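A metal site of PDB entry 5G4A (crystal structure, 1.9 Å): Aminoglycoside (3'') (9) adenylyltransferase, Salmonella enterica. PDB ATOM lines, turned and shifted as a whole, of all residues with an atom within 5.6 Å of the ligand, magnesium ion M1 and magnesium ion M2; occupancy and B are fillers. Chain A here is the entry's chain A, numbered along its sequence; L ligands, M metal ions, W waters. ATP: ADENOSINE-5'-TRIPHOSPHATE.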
ATOM      1  N   TYR A  34      25.968  -8.847  -0.986  1.00  0.00           N
ATOM      2  CA  TYR A  34      24.825  -9.749  -1.002  1.00  0.00           C
ATOM      3  C   TYR A  34      24.025  -9.513   0.286  1.00  0.00           C
ATOM      4  O   TYR A  34      24.239  -8.533   0.999  1.00  0.00           O
ATOM      5  CB  TYR A  34      25.297 -11.210  -1.160  1.00  0.00           C
ATOM      6  CG  TYR A  34      25.993 -11.743   0.073  1.00  0.00           C
ATOM      7  CD1 TYR A  34      27.330 -11.396   0.367  1.00  0.00           C
ATOM      8  CD2 TYR A  34      25.333 -12.561   0.962  1.00  0.00           C
ATOM      9  CE1 TYR A  34      27.965 -11.897   1.515  1.00  0.00           C
ATOM     10  CE2 TYR A  34      25.933 -13.026   2.114  1.00  0.00           C
ATOM     11  CZ  TYR A  34      27.248 -12.720   2.379  1.00  0.00           C
ATOM     12  OH  TYR A  34      27.819 -13.214   3.529  1.00  0.00           O
ATOM     13  N   GLY A  35      23.110 -10.437   0.606  1.00  0.00           N
ATOM     14  CA  GLY A  35      22.344 -10.323   1.839  1.00  0.00           C
ATOM     15  C   GLY A  35      21.299  -9.219   1.714  1.00  0.00           C
ATOM     16  O   GLY A  35      20.939  -8.792   0.605  1.00  0.00           O
ATOM     17  N   SER A  36      20.800  -8.751   2.861  1.00  0.00           N
ATOM     18  CA  SER A  36      19.552  -7.980   2.823  1.00  0.00           C
ATOM     19  C   SER A  36      19.721  -6.610   2.163  1.00  0.00           C
ATOM     20  O   SER A  36      18.723  -6.038   1.721  1.00  0.00           O
ATOM     21  CB  SER A  36      18.975  -7.817   4.236  1.00  0.00           C
ATOM     22  OG  SER A  36      19.793  -7.031   5.092  1.00  0.00           O
ATOM     23  N   ALA A  37      20.939  -6.075   2.079  1.00  0.00           N
ATOM     24  CA  ALA A  37      21.121  -4.817   1.358  1.00  0.00           C
ATOM     25  C   ALA A  37      20.688  -4.943  -0.103  1.00  0.00           C
ATOM     26  O   ALA A  37      20.214  -3.969  -0.704  1.00  0.00           O
ATOM     27  CB  ALA A  37      22.583  -4.379   1.432  1.00  0.00           C
ATOM     28  N   GLY A  40      16.777  -7.504   0.050  1.00  0.00           N
ATOM     29  CA  GLY A  40      15.600  -6.992   0.719  1.00  0.00           C
ATOM     30  C   GLY A  40      15.575  -7.205   2.215  1.00  0.00           C
ATOM     31  O   GLY A  40      16.071  -8.217   2.710  1.00  0.00           O
ATOM     32  N   GLY A  41      14.997  -6.244   2.946  1.00  0.00           N
ATOM     33  CA  GLY A  41      14.847  -6.379   4.376  1.00  0.00           C
ATOM     34  C   GLY A  41      15.983  -5.745   5.136  1.00  0.00           C
ATOM     35  O   GLY A  41      16.456  -6.283   6.143  1.00  0.00           O
ATOM     36  N   LEU A  42      16.443  -4.585   4.662  1.00  0.00           N
ATOM     37  CA  LEU A  42      17.525  -3.876   5.324  1.00  0.00           C
ATOM     38  C   LEU A  42      16.945  -3.094   6.502  1.00  0.00           C
ATOM     39  O   LEU A  42      16.247  -2.105   6.299  1.00  0.00           O
ATOM     40  CB  LEU A  42      18.230  -2.952   4.341  1.00  0.00           C
ATOM     41  CG  LEU A  42      19.434  -2.231   4.923  1.00  0.00           C
ATOM     42  CD1 LEU A  42      20.601  -3.211   4.997  1.00  0.00           C
ATOM     43  CD2 LEU A  42      19.752  -1.073   4.027  1.00  0.00           C
ATOM     44  N   LYS A  43      17.205  -3.549   7.706  1.00  0.00           N
ATOM     45  CA  LYS A  43      16.671  -2.987   8.939  1.00  0.00           C
ATOM     46  C   LYS A  43      17.719  -2.121   9.617  1.00  0.00           C
ATOM     47  O   LYS A  43      18.898  -2.150   9.254  1.00  0.00           O
ATOM     48  CB  LYS A  43      16.246  -4.127   9.884  1.00  0.00           C
ATOM     49  CG  LYS A  43      15.302  -5.103   9.225  1.00  0.00           C
ATOM     50  CD  LYS A  43      14.023  -4.373   8.849  1.00  0.00           C
ATOM     51  CE  LYS A  43      12.971  -5.321   8.386  1.00  0.00           C
ATOM     52  NZ  LYS A  43      11.696  -4.599   8.182  1.00  0.00           N
ATOM     53  N   SER A  46      20.650  -4.064  10.607  1.00  0.00           N
ATOM     54  CA  SER A  46      21.197  -4.975   9.612  1.00  0.00           C
ATOM     55  C   SER A  46      22.649  -4.636   9.290  1.00  0.00           C
ATOM     56  O   SER A  46      23.039  -3.462   9.281  1.00  0.00           O
ATOM     57  CB  SER A  46      20.339  -4.952   8.342  1.00  0.00           C
ATOM     58  OG  SER A  46      19.061  -5.509   8.612  1.00  0.00           O
ATOM     59  N   ASP A  47      23.452  -5.672   9.046  1.00  0.00           N
ATOM     60  CA  ASP A  47      24.825  -5.498   8.625  1.00  0.00           C
ATOM     61  C   ASP A  47      24.893  -5.274   7.103  1.00  0.00           C
ATOM     62  O   ASP A  47      23.891  -5.315   6.405  1.00  0.00           O
ATOM     63  CB  ASP A  47      25.652  -6.718   9.044  1.00  0.00           C
ATOM     64  CG  ASP A  47      25.113  -8.035   8.480  1.00  0.00           C
ATOM     65  OD1 ASP A  47      24.206  -8.010   7.616  1.00  0.00           O
ATOM     66  OD2 ASP A  47      25.602  -9.110   8.892  1.00  0.00           O
ATOM     67  N   ILE A  48      26.106  -5.037   6.598  1.00  0.00           N
ATOM     68  CA  ILE A  48      26.410  -5.010   5.167  1.00  0.00           C
ATOM     69  C   ILE A  48      27.219  -6.254   4.850  1.00  0.00           C
ATOM     70  O   ILE A  48      28.348  -6.405   5.354  1.00  0.00           O
ATOM     71  CB  ILE A  48      27.175  -3.736   4.761  1.00  0.00           C
ATOM     72  CG1 ILE A  48      26.353  -2.468   5.023  1.00  0.00           C
ATOM     73  CG2 ILE A  48      27.599  -3.817   3.272  1.00  0.00           C
ATOM     74  CD1 ILE A  48      27.137  -1.155   4.789  1.00  0.00           C
ATOM     75  N   ASP A  49      26.674  -7.165   4.041  1.00  0.00           N
ATOM     76  CA  ASP A  49      27.297  -8.477   3.810  1.00  0.00           C
ATOM     77  C   ASP A  49      28.164  -8.447   2.568  1.00  0.00           C
ATOM     78  O   ASP A  49      27.689  -8.077   1.485  1.00  0.00           O
ATOM     79  CB  ASP A  49      26.238  -9.574   3.675  1.00  0.00           C
ATOM     80  CG  ASP A  49      25.431  -9.811   4.946  1.00  0.00           C
ATOM     81  OD1 ASP A  49      26.011 -10.332   5.930  1.00  0.00           O
ATOM     82  OD2 ASP A  49      24.218  -9.531   4.961  1.00  0.00           O
ATOM     83  N   GLU A  87      30.100  -7.282   7.606  1.00  0.00           N
ATOM     84  CA  GLU A  87      30.541  -8.667   7.656  1.00  0.00           C
ATOM     85  C   GLU A  87      31.327  -8.945   6.393  1.00  0.00           C
ATOM     86  O   GLU A  87      30.793  -8.783   5.291  1.00  0.00           O
ATOM     87  CB  GLU A  87      29.388  -9.650   7.802  1.00  0.00           C
ATOM     88  CG  GLU A  87      29.856 -11.103   7.833  1.00  0.00           C
ATOM     89  CD  GLU A  87      28.723 -12.096   8.052  1.00  0.00           C
ATOM     90  OE1 GLU A  87      27.599 -11.669   8.376  1.00  0.00           O
ATOM     91  OE2 GLU A  87      28.964 -13.313   7.889  1.00  0.00           O
ATOM     92  N   ASP A 130      28.377 -23.089   5.947  1.00  0.00           N
ATOM     93  CA  ASP A 130      27.571 -21.931   5.511  1.00  0.00           C
ATOM     94  C   ASP A 130      28.086 -21.319   4.207  1.00  0.00           C
ATOM     95  O   ASP A 130      27.298 -20.692   3.486  1.00  0.00           O
ATOM     96  CB  ASP A 130      27.519 -20.867   6.607  1.00  0.00           C
ATOM     97  CG  ASP A 130      26.526 -19.790   6.285  1.00  0.00           C
ATOM     98  OD1 ASP A 130      25.322 -20.117   6.167  1.00  0.00           O
ATOM     99  OD2 ASP A 130      26.947 -18.623   6.120  1.00  0.00           O
ATOM    100  N   LEU A 133      25.867 -22.046   1.459  1.00  0.00           N
ATOM    101  CA  LEU A 133      24.690 -21.191   1.439  1.00  0.00           C
ATOM    102  C   LEU A 133      25.027 -19.791   0.916  1.00  0.00           C
ATOM    103  O   LEU A 133      24.275 -19.219   0.128  1.00  0.00           O
ATOM    104  CB  LEU A 133      24.077 -21.107   2.837  1.00  0.00           C
ATOM    105  CG  LEU A 133      23.780 -22.405   3.615  1.00  0.00           C
ATOM    106  CD1 LEU A 133      22.869 -22.088   4.794  1.00  0.00           C
ATOM    107  CD2 LEU A 133      23.142 -23.471   2.756  1.00  0.00           C
ATOM    108  N   LEU A 134      26.160 -19.224   1.361  1.00  0.00           N
ATOM    109  CA  LEU A 134      26.559 -17.894   0.907  1.00  0.00           C
ATOM    110  C   LEU A 134      26.645 -17.830  -0.621  1.00  0.00           C
ATOM    111  O   LEU A 134      25.987 -16.995  -1.255  1.00  0.00           O
ATOM    112  CB  LEU A 134      27.891 -17.487   1.548  1.00  0.00           C
ATOM    113  CG  LEU A 134      27.872 -17.260   3.067  1.00  0.00           C
ATOM    114  CD1 LEU A 134      29.162 -16.567   3.507  1.00  0.00           C
ATOM    115  CD2 LEU A 134      26.618 -16.461   3.481  1.00  0.00           C
ATOM    116  N   GLN A 137      23.328 -18.131  -2.341  1.00  0.00           N
ATOM    117  CA  GLN A 137      22.566 -16.883  -2.274  1.00  0.00           C
ATOM    118  C   GLN A 137      23.130 -15.838  -3.216  1.00  0.00           C
ATOM    119  O   GLN A 137      22.372 -15.083  -3.844  1.00  0.00           O
ATOM    120  CB  GLN A 137      22.566 -16.351  -0.846  1.00  0.00           C
ATOM    121  CG  GLN A 137      21.548 -17.061  -0.036  1.00  0.00           C
ATOM    122  CD  GLN A 137      21.735 -16.827   1.413  1.00  0.00           C
ATOM    123  OE1 GLN A 137      22.451 -17.582   2.074  1.00  0.00           O
ATOM    124  NE2 GLN A 137      21.119 -15.771   1.935  1.00  0.00           N
ATOM    125  N   LEU A 166      22.163 -26.827   4.365  1.00  0.00           N
ATOM    126  CA  LEU A 166      20.967 -26.242   4.958  1.00  0.00           C
ATOM    127  C   LEU A 166      20.620 -26.899   6.289  1.00  0.00           C
ATOM    128  O   LEU A 166      20.191 -26.235   7.230  1.00  0.00           O
ATOM    129  CB  LEU A 166      19.791 -26.386   3.990  1.00  0.00           C
ATOM    130  CG  LEU A 166      19.799 -25.359   2.874  1.00  0.00           C
ATOM    131  CD1 LEU A 166      18.854 -25.851   1.797  1.00  0.00           C
ATOM    132  CD2 LEU A 166      19.341 -24.006   3.457  1.00  0.00           C
ATOM    133  N   PRO A 169      23.115 -26.694  10.475  1.00  0.00           N
ATOM    134  CA  PRO A 169      22.894 -25.956  11.728  1.00  0.00           C
ATOM    135  C   PRO A 169      21.834 -26.567  12.626  1.00  0.00           C
ATOM    136  O   PRO A 169      21.751 -26.182  13.798  1.00  0.00           O
ATOM    137  CB  PRO A 169      22.467 -24.563  11.264  1.00  0.00           C
ATOM    138  CG  PRO A 169      22.934 -24.472   9.843  1.00  0.00           C
ATOM    139  CD  PRO A 169      22.804 -25.862   9.297  1.00  0.00           C
ATOM    140  N   THR A 189      16.096 -18.076  11.604  1.00  0.00           N
ATOM    141  CA  THR A 189      16.934 -18.864  10.693  1.00  0.00           C
ATOM    142  C   THR A 189      16.277 -20.197  10.372  1.00  0.00           C
ATOM    143  O   THR A 189      16.324 -20.660   9.218  1.00  0.00           O
ATOM    144  CB  THR A 189      18.301 -19.101  11.316  1.00  0.00           C
ATOM    145  OG1 THR A 189      18.892 -17.854  11.674  1.00  0.00           O
ATOM    146  CG2 THR A 189      19.225 -19.849  10.315  1.00  0.00           C
ATOM    147  N   ARG A 192      13.819 -19.669   7.771  1.00  0.00           N
ATOM    148  CA  ARG A 192      14.419 -19.551   6.442  1.00  0.00           C
ATOM    149  C   ARG A 192      14.855 -20.902   5.904  1.00  0.00           C
ATOM    150  O   ARG A 192      14.692 -21.188   4.706  1.00  0.00           O
ATOM    151  CB  ARG A 192      15.626 -18.614   6.464  1.00  0.00           C
ATOM    152  CG  ARG A 192      15.300 -17.184   6.842  1.00  0.00           C
ATOM    153  CD  ARG A 192      16.578 -16.325   6.797  1.00  0.00           C
ATOM    154  NE  ARG A 192      16.761 -15.681   5.511  1.00  0.00           N
ATOM    155  CZ  ARG A 192      17.765 -14.862   5.233  1.00  0.00           C
ATOM    156  NH1 ARG A 192      18.703 -14.614   6.144  1.00  0.00           N
ATOM    157  NH2 ARG A 192      17.861 -14.292   4.044  1.00  0.00           N
ATOM    158  N   ILE A 193      15.454 -21.729   6.760  1.00  0.00           N
ATOM    159  CA  ILE A 193      15.874 -23.069   6.337  1.00  0.00           C
ATOM    160  C   ILE A 193      14.669 -23.854   5.858  1.00  0.00           C
ATOM    161  O   ILE A 193      14.704 -24.509   4.803  1.00  0.00           O
ATOM    162  CB  ILE A 193      16.591 -23.806   7.489  1.00  0.00           C
ATOM    163  CG1 ILE A 193      18.003 -23.223   7.706  1.00  0.00           C
ATOM    164  CG2 ILE A 193      16.681 -25.328   7.196  1.00  0.00           C
ATOM    165  CD1 ILE A 193      18.601 -23.543   9.088  1.00  0.00           C
ATOM    166  N   THR A 196      13.526 -22.529   2.459  1.00  0.00           N
ATOM    167  CA  THR A 196      14.400 -22.949   1.353  1.00  0.00           C
ATOM    168  C   THR A 196      14.223 -24.421   1.022  1.00  0.00           C
ATOM    169  O   THR A 196      14.200 -24.794  -0.158  1.00  0.00           O
ATOM    170  CB  THR A 196      15.870 -22.623   1.674  1.00  0.00           C
ATOM    171  OG1 THR A 196      16.005 -21.216   1.908  1.00  0.00           O
ATOM    172  CG2 THR A 196      16.781 -22.987   0.495  1.00  0.00           C
ATOM    173  N   PHE A 202      15.412 -18.620  -1.649  1.00  0.00           N
ATOM    174  CA  PHE A 202      15.830 -17.845  -0.487  1.00  0.00           C
ATOM    175  C   PHE A 202      14.938 -16.624  -0.325  1.00  0.00           C
ATOM    176  O   PHE A 202      14.457 -16.058  -1.308  1.00  0.00           O
ATOM    177  CB  PHE A 202      17.308 -17.444  -0.604  1.00  0.00           C
ATOM    178  CG  PHE A 202      18.226 -18.625  -0.616  1.00  0.00           C
ATOM    179  CD1 PHE A 202      18.518 -19.269  -1.803  1.00  0.00           C
ATOM    180  CD2 PHE A 202      18.704 -19.145   0.575  1.00  0.00           C
ATOM    181  CE1 PHE A 202      19.323 -20.393  -1.802  1.00  0.00           C
ATOM    182  CE2 PHE A 202      19.531 -20.267   0.588  1.00  0.00           C
ATOM    183  CZ  PHE A 202      19.837 -20.890  -0.611  1.00  0.00           C
ATOM    184  N   THR A 203      14.698 -16.228   0.927  1.00  0.00           N
ATOM    185  CA  THR A 203      13.811 -15.101   1.178  1.00  0.00           C
ATOM    186  C   THR A 203      14.246 -14.459   2.477  1.00  0.00           C
ATOM    187  O   THR A 203      15.034 -15.030   3.245  1.00  0.00           O
ATOM    188  CB  THR A 203      12.327 -15.535   1.214  1.00  0.00           C
ATOM    189  OG1 THR A 203      11.482 -14.392   1.034  1.00  0.00           O
ATOM    190  CG2 THR A 203      11.995 -16.192   2.546  1.00  0.00           C
ATOM    191  N   SER A 204      13.728 -13.256   2.727  1.00  0.00           N
ATOM    192  CA  SER A 204      14.124 -12.496   3.903  1.00  0.00           C
ATOM    193  C   SER A 204      13.658 -13.192   5.170  1.00  0.00           C
ATOM    194  O   SER A 204      12.749 -14.031   5.167  1.00  0.00           O
ATOM    195  CB  SER A 204      13.542 -11.084   3.862  1.00  0.00           C
ATOM    196  OG  SER A 204      12.132 -11.121   3.981  1.00  0.00           O
ATOM    197  N   LYS A 205      14.290 -12.807   6.281  1.00  0.00           N
ATOM    198  CA  LYS A 205      13.883 -13.320   7.588  1.00  0.00           C
ATOM    199  C   LYS A 205      12.404 -13.073   7.835  1.00  0.00           C
ATOM    200  O   LYS A 205      11.692 -13.948   8.335  1.00  0.00           O
ATOM    201  CB  LYS A 205      14.738 -12.655   8.676  1.00  0.00           C
ATOM    202  CG  LYS A 205      16.159 -13.231   8.729  1.00  0.00           C
ATOM    203  CD  LYS A 205      17.123 -12.240   9.407  1.00  0.00           C
ATOM    204  CE  LYS A 205      18.574 -12.772   9.394  1.00  0.00           C
ATOM    205  NZ  LYS A 205      19.436 -11.863  10.219  1.00  0.00           N
ATOM    206  N   TYR A 231      12.539  -8.880  15.911  1.00  0.00           N
ATOM    207  CA  TYR A 231      13.478  -8.571  14.841  1.00  0.00           C
ATOM    208  C   TYR A 231      13.017  -7.329  14.077  1.00  0.00           C
ATOM    209  O   TYR A 231      13.833  -6.477  13.711  1.00  0.00           O
ATOM    210  CB  TYR A 231      13.603  -9.777  13.901  1.00  0.00           C
ATOM    211  CG  TYR A 231      14.501  -9.507  12.713  1.00  0.00           C
ATOM    212  CD1 TYR A 231      15.892  -9.607  12.828  1.00  0.00           C
ATOM    213  CD2 TYR A 231      13.958  -9.125  11.502  1.00  0.00           C
ATOM    214  CE1 TYR A 231      16.703  -9.352  11.741  1.00  0.00           C
ATOM    215  CE2 TYR A 231      14.762  -8.864  10.418  1.00  0.00           C
ATOM    216  CZ  TYR A 231      16.131  -8.974  10.539  1.00  0.00           C
ATOM    217  OH  TYR A 231      16.915  -8.693   9.430  1.00  0.00           O
HETATM  218  PG  ATP L   1      20.020  -8.930   8.179  1.00  0.00           P
HETATM  219  O1G ATP L   1      21.528  -8.883   8.175  1.00  0.00           O
HETATM  220  O2G ATP L   1      19.375  -9.213   9.531  1.00  0.00           O
HETATM  221  O3G ATP L   1      19.346  -7.704   7.524  1.00  0.00           O
HETATM  222  PB  ATP L   1      20.341 -10.995   6.172  1.00  0.00           P
HETATM  223  O1B ATP L   1      21.366 -10.165   5.526  1.00  0.00           O
HETATM  224  O2B ATP L   1      19.363 -11.651   5.218  1.00  0.00           O
HETATM  225  O3B ATP L   1      19.537 -10.135   7.249  1.00  0.00           O
HETATM  226  PA  ATP L   1      22.459 -12.204   7.797  1.00  0.00           P
HETATM  227  O1A ATP L   1      23.399 -11.105   7.382  1.00  0.00           O
HETATM  228  O2A ATP L   1      22.155 -12.200   9.265  1.00  0.00           O
HETATM  229  O3A ATP L   1      21.049 -12.126   7.046  1.00  0.00           O
HETATM  230  O5' ATP L   1      23.013 -13.618   7.311  1.00  0.00           O
HETATM  231  C5' ATP L   1      22.155 -14.771   7.418  1.00  0.00           C
HETATM  232  C4' ATP L   1      23.005 -15.979   7.689  1.00  0.00           C
HETATM  233  O4' ATP L   1      22.139 -17.121   7.856  1.00  0.00           O
HETATM  234  C3' ATP L   1      23.979 -16.354   6.550  1.00  0.00           C
HETATM  235  O3' ATP L   1      25.195 -16.891   7.067  1.00  0.00           O
HETATM  236  C2' ATP L   1      23.163 -17.384   5.770  1.00  0.00           C
HETATM  237  O2' ATP L   1      23.956 -18.255   4.974  1.00  0.00           O
HETATM  238  C1' ATP L   1      22.507 -18.133   6.932  1.00  0.00           C
HETATM  239  N9  ATP L   1      21.342 -18.929   6.581  1.00  0.00           N
HETATM  240  C8  ATP L   1      21.107 -20.216   6.991  1.00  0.00           C
HETATM  241  N7  ATP L   1      20.097 -20.794   6.379  1.00  0.00           N
HETATM  242  C5  ATP L   1      19.613 -19.802   5.534  1.00  0.00           C
HETATM  243  C6  ATP L   1      18.573 -19.804   4.578  1.00  0.00           C
HETATM  244  N6  ATP L   1      17.814 -20.864   4.291  1.00  0.00           N
HETATM  245  N1  ATP L   1      18.358 -18.664   3.883  1.00  0.00           N
HETATM  246  C2  ATP L   1      19.146 -17.600   4.129  1.00  0.00           C
HETATM  247  N3  ATP L   1      20.168 -17.499   4.987  1.00  0.00           N
HETATM  248  C4  ATP L   1      20.355 -18.643   5.657  1.00  0.00           C
HETATM  249 MG    MG M   1      25.640 -11.028   7.968  1.00  0.00          MG
HETATM  250 MG    MG M   2      22.913  -9.120   6.537  1.00  0.00          MG
HETATM  251  O   HOH W   1      16.149  -8.879   6.958  1.00  0.00           O
HETATM  252  O   HOH W   2      19.447 -16.282   8.423  1.00  0.00           O
HETATM  253  O   HOH W   3      21.087 -14.168   4.100  1.00  0.00           O
HETATM  254  O   HOH W   4      23.276 -12.484   4.381  1.00  0.00           O
HETATM  255  O   HOH W   5      16.940 -10.935   2.802  1.00  0.00           O
HETATM  256  O   HOH W   6      25.947 -13.000   5.531  1.00  0.00           O
HETATM  257  O   HOH W   7      18.769  -6.503  11.319  1.00  0.00           O
HETATM  258  O   HOH W   8      16.657 -11.057   5.574  1.00  0.00           O
HETATM  259  O   HOH W   9      25.057 -12.141  10.087  1.00  0.00           O
HETATM  260  O   HOH W  10      20.376  -8.292  11.989  1.00  0.00           O
HETATM  261  O   HOH W  11      22.722  -8.898  10.621  1.00  0.00           O
HETATM  262  O   HOH W  12      22.427  -7.275   5.628  1.00  0.00           O
HETATM  263  O   HOH W  13      25.176 -18.208   9.644  1.00  0.00           O
HETATM  264  O   HOH W  14      19.470 -11.896   2.539  1.00  0.00           O
HETATM  265  O   HOH W  15      15.696 -18.373   2.851  1.00  0.00           O
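Magnesium ion M1 is bound by the side-chain carboxylate of Glu 87 (2.1 Å), the side-chain carboxylate of Asp 47 (2.1 Å), the side-chain carboxylate of Asp 49 (2.2 Å), an oxygen (O1A) of the ligand (2.3 Å) and water W9 (2.5 Å).
Magnesium ion M1 has five donor atoms within binding distance.
Magnesium ion M2 is bound by the side-chain carboxylate (OD1) of Asp 47 (2.0 Å).
OD2 of Asp 49 binds magnesium ion M2.
Water W12 is bound to magnesium ion M2 (2.1 Å).
Magnesium ion M2 is bound by O1B of the ligand.
O1G of the ligand is bound to magnesium ion M2, 2.2 Å away.
Magnesium ion M2 is bound by an oxygen (O1A) of the ligand (2.2 Å).
Magnesium ion M2 has six donor atoms within binding distance.
Water W12 bridges O of Asp 47 (2.6 Å) and OG of Ser 36 (2.7 Å).
Water W14 lies within hydrogen-bond range of O2B of the ligand, NH2 of Arg 192 and N of Ser 36.
Water W8 lies within hydrogen-bond range of O2B of the ligand and N of Lys 205.
Water W2 lies within hydrogen-bond range of O4' of the ligand (2.9 Å) and NH1 of Arg 192 (2.9 Å).
Water W6 lies within hydrogen-bond range of the side-chain hydroxyl (OH) of Tyr 34 and an oxygen (O5') of the ligand.
Water W7 lies within hydrogen-bond range of the side-chain hydroxyl (OG) of Ser 46 (2.9 Å), an oxygen (O2G) of the ligand (3.3 Å) and the side-chain hydroxyl (OH) of Tyr 231 (3.4 Å).
Three residues have an atom within 4 Å of magnesium ion M1: Asp 47, Asp 49 and Glu 87.
The nearest printed residue that does not touch magnesium ion M1 is Tyr 34 (5.4 Å).
The side-chain hydroxyl of Ser 46 is in hydrogen-bond range of an oxygen (O3G) of the ligand, 2.5 Å away.
OH of Tyr 231 is in hydrogen-bond range of O2G of the ligand (2.5 Å).
An oxygen (O1B) of the ligand lies close to the backbone NH (N) of Ser 36 (3.1 Å).
OG of Ser 36 sits at hydrogen-bond distance from O3G of the ligand (2.6 Å).
An oxygen (O2') of the ligand lies within hydrogen-bond range of the side-chain carboxylate (OD1) of Asp 130 (2.6 Å).
O2G of the ligand lies within salt-bridge range of NZ of Lys 205 (2.7 Å).
The side-chain hydroxyl of Thr 196 sits at hydrogen-bond distance from a nitrogen (N6) of the ligand (3.0 Å).
A nitrogen (N6) of the ligand lies within hydrogen-bond range of the backbone carbonyl oxygen (O) of Arg 192 (3.2 Å).
The guanidinium group (NH1) of Arg 192 lies within salt-bridge range of an oxygen (O2B) of the ligand (3.2 Å).
An oxygen (O2') of the ligand is in hydrogen-bond range of the side-chain amide oxygen of Gln 137 (3.3 Å).
O of Asp 49 lies within hydrogen-bond range of N of Tyr 34.
The backbone carbonyl oxygen of Ile 48 lies within hydrogen-bond range of the backbone NH of Glu 87.
N of Lys 43 lies within hydrogen-bond range of OG of Ser 46, at 2.8 Å.
The side-chain hydroxyl (OG1) of Thr 196 sits at hydrogen-bond distance from the backbone carbonyl oxygen (O) of Arg 192.
The backbone carbonyl oxygen of Thr 203 sits at hydrogen-bond distance from the guanidinium group of Arg 192, 2.9 Å away.
OE1 of Gln 137 sits close to O of Leu 133, at 3.1 Å.
Of the 28 residues printed, 2 come within 4 Å of magnesium ion M2.
The nearest printed residue that does not touch magnesium ion M2 is Ser 36 (4.02 Å).
Gly 35 touches the ligand (CA to O1B, 3.8 Å).
Gly 41 touches the ligand (O to O3G, 3.5 Å).
Leu 133 touches the ligand.
Leu 134 touches the ligand (CD2 to O2', 3.5 Å).
Leu 166 touches the ligand.
Thr 189 touches the ligand (CG2 to C8, 3.8 Å).
CG1 of Ile 193 touches N7 of the ligand (3.5 Å).
Phe 202 touches the ligand (CD2 to N1, 3.4 Å).
Within 4 Å of the ligand: Gly 35, Ser 36, Gly 41, Ser 46, Asp 47, Asp 49, Asp 130, Leu 133, Leu 134, Gln 137, Leu 166, Thr 189, Arg 192, Ile 193, Thr 196, Phe 202, Lys 205 and Tyr 231.
The nearest printed residue that does not touch the ligand is Glu 87 (4.4 Å).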
